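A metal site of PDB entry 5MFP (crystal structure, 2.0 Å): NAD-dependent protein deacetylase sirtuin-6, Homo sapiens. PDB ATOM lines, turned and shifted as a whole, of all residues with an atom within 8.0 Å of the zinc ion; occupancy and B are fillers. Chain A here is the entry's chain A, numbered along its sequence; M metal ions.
The side-chain hydroxyl (OG1) of Thr 140 lies close to the side-chain sulfur (SG) of Cys 138 (3.1 Å). The backbone NH of Lys 137 lies close to the side-chain sulfur of Cys 135, at 3.2 Å. The backbone NH (N) of Cys 135 sits at hydrogen-bond distance from the backbone carbonyl oxygen (O) of Thr 140, 2.9 Å away. The backbone NH of Cys 160 lies within hydrogen-bond range of the backbone carbonyl oxygen of Gly 173 (2.9 Å). SG of Cys 160 sits close to N of Val 162 (3.7 Å). The backbone NH of Arg 172 sits at hydrogen-bond distance from the backbone carbonyl oxygen of Cys 160 (3.2 Å). The backbone NH of Gly 173 lies close to the side-chain sulfur of Cys 171. The backbone NH (N) of Cys 171 is in hydrogen-bond range of the backbone carbonyl oxygen (O) of Val 162 (3.2 Å).
Of the 19 residues printed, 4 come within 4 Å of the zinc ion.
The zinc ion is bound by SG of Cys 138 (2.3 Å), SG of Cys 135 (2.3 Å), SG of Cys 160 (2.3 Å) and SG of Cys 171 (2.4 Å). The zinc ion has four donor atoms within binding distance.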
ATOM      1  N   GLU A 134      16.049 -24.093  19.424  1.00  0.00           N
ATOM      2  CA  GLU A 134      15.694 -25.511  19.507  1.00  0.00           C
ATOM      3  C   GLU A 134      14.250 -25.785  18.991  1.00  0.00           C
ATOM      4  O   GLU A 134      13.357 -25.025  19.299  1.00  0.00           O
ATOM      5  CB  GLU A 134      15.806 -25.963  20.953  1.00  0.00           C
ATOM      6  CG  GLU A 134      15.370 -27.405  21.179  1.00  0.00           C
ATOM      7  CD  GLU A 134      15.705 -27.964  22.543  1.00  0.00           C
ATOM      8  OE1 GLU A 134      16.871 -27.836  23.024  1.00  0.00           O
ATOM      9  OE2 GLU A 134      14.820 -28.643  23.105  1.00  0.00           O
ATOM     10  N   CYS A 135      14.061 -26.849  18.180  1.00  0.00           N
ATOM     11  CA  CYS A 135      12.735 -27.193  17.650  1.00  0.00           C
ATOM     12  C   CYS A 135      11.899 -27.780  18.806  1.00  0.00           C
ATOM     13  O   CYS A 135      12.240 -28.801  19.397  1.00  0.00           O
ATOM     14  CB  CYS A 135      12.801 -28.215  16.518  1.00  0.00           C
ATOM     15  SG  CYS A 135      11.188 -28.705  15.803  1.00  0.00           S
ATOM     16  N   ALA A 136      10.850 -27.071  19.146  1.00  0.00           N
ATOM     17  CA  ALA A 136       9.830 -27.596  20.083  1.00  0.00           C
ATOM     18  C   ALA A 136       9.274 -28.990  19.643  1.00  0.00           C
ATOM     19  O   ALA A 136       8.948 -29.846  20.489  1.00  0.00           O
ATOM     20  CB  ALA A 136       8.730 -26.568  20.187  1.00  0.00           C
ATOM     21  N   LYS A 137       9.285 -29.293  18.341  1.00  0.00           N
ATOM     22  CA  LYS A 137       8.724 -30.566  17.860  1.00  0.00           C
ATOM     23  C   LYS A 137       9.679 -31.715  17.844  1.00  0.00           C
ATOM     24  O   LYS A 137       9.412 -32.688  18.499  1.00  0.00           O
ATOM     25  CB  LYS A 137       8.066 -30.373  16.479  1.00  0.00           C
ATOM     26  CG  LYS A 137       6.947 -29.321  16.574  1.00  0.00           C
ATOM     27  CD  LYS A 137       5.818 -29.484  15.557  1.00  0.00           C
ATOM     28  CE  LYS A 137       4.527 -28.820  16.072  1.00  0.00           C
ATOM     29  NZ  LYS A 137       3.810 -28.037  15.027  1.00  0.00           N
ATOM     30  N   CYS A 138      10.789 -31.628  17.111  1.00  0.00           N
ATOM     31  CA  CYS A 138      11.771 -32.728  17.027  1.00  0.00           C
ATOM     32  C   CYS A 138      13.007 -32.564  17.931  1.00  0.00           C
ATOM     33  O   CYS A 138      13.804 -33.469  18.016  1.00  0.00           O
ATOM     34  CB  CYS A 138      12.188 -32.930  15.591  1.00  0.00           C
ATOM     35  SG  CYS A 138      13.259 -31.645  14.885  1.00  0.00           S
ATOM     36  N   LYS A 139      13.172 -31.404  18.571  1.00  0.00           N
ATOM     37  CA  LYS A 139      14.253 -31.106  19.561  1.00  0.00           C
ATOM     38  C   LYS A 139      15.620 -30.726  18.993  1.00  0.00           C
ATOM     39  O   LYS A 139      16.572 -30.496  19.779  1.00  0.00           O
ATOM     40  CB  LYS A 139      14.405 -32.229  20.580  1.00  0.00           C
ATOM     41  CG  LYS A 139      13.083 -32.517  21.309  1.00  0.00           C
ATOM     42  CD  LYS A 139      12.807 -31.391  22.290  1.00  0.00           C
ATOM     43  CE  LYS A 139      11.330 -31.041  22.375  1.00  0.00           C
ATOM     44  NZ  LYS A 139      10.684 -31.894  23.396  1.00  0.00           N
ATOM     45  N   THR A 140      15.686 -30.635  17.666  1.00  0.00           N
ATOM     46  CA  THR A 140      16.890 -30.327  16.915  1.00  0.00           C
ATOM     47  C   THR A 140      17.313 -28.905  17.235  1.00  0.00           C
ATOM     48  O   THR A 140      16.512 -27.979  17.079  1.00  0.00           O
ATOM     49  CB  THR A 140      16.677 -30.435  15.380  1.00  0.00           C
ATOM     50  OG1 THR A 140      16.385 -31.777  15.018  1.00  0.00           O
ATOM     51  CG2 THR A 140      17.968 -29.992  14.566  1.00  0.00           C
ATOM     52  N   GLN A 141      18.598 -28.732  17.526  1.00  0.00           N
ATOM     53  CA  GLN A 141      19.198 -27.435  17.926  1.00  0.00           C
ATOM     54  C   GLN A 141      19.927 -26.800  16.739  1.00  0.00           C
ATOM     55  O   GLN A 141      20.432 -27.492  15.884  1.00  0.00           O
ATOM     56  CB  GLN A 141      20.093 -27.644  19.133  1.00  0.00           C
ATOM     57  CG  GLN A 141      19.313 -27.981  20.397  1.00  0.00           C
ATOM     58  CD  GLN A 141      20.185 -28.089  21.578  1.00  0.00           C
ATOM     59  OE1 GLN A 141      21.377 -28.263  21.476  1.00  0.00           O
ATOM     60  NE2 GLN A 141      19.606 -27.874  22.728  1.00  0.00           N
ATOM     61  N   TYR A 142      19.855 -25.491  16.622  1.00  0.00           N
ATOM     62  CA  TYR A 142      20.516 -24.784  15.544  1.00  0.00           C
ATOM     63  C   TYR A 142      21.422 -23.743  16.224  1.00  0.00           C
ATOM     64  O   TYR A 142      20.906 -22.929  17.111  1.00  0.00           O
ATOM     65  CB  TYR A 142      19.454 -24.063  14.782  1.00  0.00           C
ATOM     66  CG  TYR A 142      18.507 -24.984  14.050  1.00  0.00           C
ATOM     67  CD1 TYR A 142      17.385 -25.561  14.683  1.00  0.00           C
ATOM     68  CD2 TYR A 142      18.727 -25.294  12.653  1.00  0.00           C
ATOM     69  CE1 TYR A 142      16.503 -26.438  13.960  1.00  0.00           C
ATOM     70  CE2 TYR A 142      17.894 -26.161  11.960  1.00  0.00           C
ATOM     71  CZ  TYR A 142      16.775 -26.714  12.597  1.00  0.00           C
ATOM     72  OH  TYR A 142      15.971 -27.539  11.859  1.00  0.00           O
ATOM     73  N   LEU A 159      11.290 -21.433  11.737  1.00  0.00           N
ATOM     74  CA  LEU A 159      10.851 -22.828  11.683  1.00  0.00           C
ATOM     75  C   LEU A 159      11.981 -23.828  11.360  1.00  0.00           C
ATOM     76  O   LEU A 159      12.976 -23.550  10.663  1.00  0.00           O
ATOM     77  CB  LEU A 159       9.733 -23.025  10.626  1.00  0.00           C
ATOM     78  CG  LEU A 159       8.434 -22.276  10.889  1.00  0.00           C
ATOM     79  CD1 LEU A 159       7.443 -22.653   9.781  1.00  0.00           C
ATOM     80  CD2 LEU A 159       7.817 -22.549  12.265  1.00  0.00           C
ATOM     81  N   CYS A 160      11.754 -25.029  11.840  1.00  0.00           N
ATOM     82  CA  CYS A 160      12.641 -26.122  11.665  1.00  0.00           C
ATOM     83  C   CYS A 160      12.728 -26.600  10.193  1.00  0.00           C
ATOM     84  O   CYS A 160      11.718 -26.678   9.501  1.00  0.00           O
ATOM     85  CB  CYS A 160      12.175 -27.226  12.578  1.00  0.00           C
ATOM     86  SG  CYS A 160      13.237 -28.653  12.607  1.00  0.00           S
ATOM     87  N   THR A 161      13.944 -26.955   9.772  1.00  0.00           N
ATOM     88  CA  THR A 161      14.259 -27.326   8.421  1.00  0.00           C
ATOM     89  C   THR A 161      14.662 -28.800   8.280  1.00  0.00           C
ATOM     90  O   THR A 161      15.105 -29.192   7.227  1.00  0.00           O
ATOM     91  CB  THR A 161      15.436 -26.448   7.888  1.00  0.00           C
ATOM     92  OG1 THR A 161      16.645 -26.728   8.635  1.00  0.00           O
ATOM     93  CG2 THR A 161      15.074 -25.001   7.998  1.00  0.00           C
ATOM     94  N   VAL A 162      14.558 -29.598   9.327  1.00  0.00           N
ATOM     95  CA  VAL A 162      14.956 -30.993   9.265  1.00  0.00           C
ATOM     96  C   VAL A 162      14.117 -31.752   8.187  1.00  0.00           C
ATOM     97  O   VAL A 162      12.922 -31.474   8.064  1.00  0.00           O
ATOM     98  CB  VAL A 162      14.771 -31.706  10.638  1.00  0.00           C
ATOM     99  CG1 VAL A 162      15.018 -33.191  10.537  1.00  0.00           C
ATOM    100  CG2 VAL A 162      15.728 -31.161  11.656  1.00  0.00           C
ATOM    101  N   ALA A 163      14.766 -32.716   7.483  1.00  0.00           N
ATOM    102  CA  ALA A 163      14.267 -33.421   6.253  1.00  0.00           C
ATOM    103  C   ALA A 163      12.830 -33.938   6.325  1.00  0.00           C
ATOM    104  O   ALA A 163      12.573 -35.029   6.831  1.00  0.00           O
ATOM    105  CB  ALA A 163      15.233 -34.571   5.836  1.00  0.00           C
ATOM    106  N   CYS A 171       9.898 -30.731   8.871  1.00  0.00           N
ATOM    107  CA  CYS A 171       9.334 -30.652  10.215  1.00  0.00           C
ATOM    108  C   CYS A 171       8.465 -29.394  10.419  1.00  0.00           C
ATOM    109  O   CYS A 171       7.335 -29.458  10.922  1.00  0.00           O
ATOM    110  CB  CYS A 171      10.449 -30.717  11.255  1.00  0.00           C
ATOM    111  SG  CYS A 171       9.912 -30.466  12.975  1.00  0.00           S
ATOM    112  N   ARG A 172       9.015 -28.244  10.086  1.00  0.00           N
ATOM    113  CA  ARG A 172       8.324 -26.980  10.338  1.00  0.00           C
ATOM    114  C   ARG A 172       7.913 -26.720  11.807  1.00  0.00           C
ATOM    115  O   ARG A 172       7.166 -25.796  12.087  1.00  0.00           O
ATOM    116  CB  ARG A 172       7.125 -26.827   9.371  1.00  0.00           C
ATOM    117  CG  ARG A 172       7.471 -27.398   7.993  1.00  0.00           C
ATOM    118  CD  ARG A 172       6.699 -26.773   6.842  1.00  0.00           C
ATOM    119  NE  ARG A 172       7.099 -25.387   6.560  1.00  0.00           N
ATOM    120  CZ  ARG A 172       6.369 -24.290   6.804  1.00  0.00           C
ATOM    121  NH1 ARG A 172       5.153 -24.348   7.364  1.00  0.00           N
ATOM    122  NH2 ARG A 172       6.857 -23.103   6.476  1.00  0.00           N
ATOM    123  N   GLY A 173       8.500 -27.459  12.757  1.00  0.00           N
ATOM    124  CA  GLY A 173       8.272 -27.190  14.167  1.00  0.00           C
ATOM    125  C   GLY A 173       8.716 -25.765  14.507  1.00  0.00           C
ATOM    126  O   GLY A 173       9.562 -25.215  13.766  1.00  0.00           O
ATOM    127  N   GLU A 174       8.157 -25.175  15.574  1.00  0.00           N
ATOM    128  CA  GLU A 174       8.387 -23.755  15.907  1.00  0.00           C
ATOM    129  C   GLU A 174       9.760 -23.750  16.596  1.00  0.00           C
ATOM    130  O   GLU A 174       9.983 -24.596  17.461  1.00  0.00           O
ATOM    131  CB  GLU A 174       7.355 -23.162  16.889  1.00  0.00           C
ATOM    132  N   LEU A 175      10.687 -22.868  16.168  1.00  0.00           N
ATOM    133  CA  LEU A 175      11.987 -22.766  16.864  1.00  0.00           C
ATOM    134  C   LEU A 175      11.810 -21.904  18.086  1.00  0.00           C
ATOM    135  O   LEU A 175      11.169 -20.844  18.008  1.00  0.00           O
ATOM    136  CB  LEU A 175      13.106 -22.183  15.985  1.00  0.00           C
ATOM    137  CG  LEU A 175      13.413 -23.014  14.725  1.00  0.00           C
ATOM    138  CD1 LEU A 175      14.689 -22.561  13.992  1.00  0.00           C
ATOM    139  CD2 LEU A 175      13.459 -24.511  15.011  1.00  0.00           C
HETATM  140 ZN    ZN M   1      11.976 -29.952  14.060  1.00  0.00          ZN
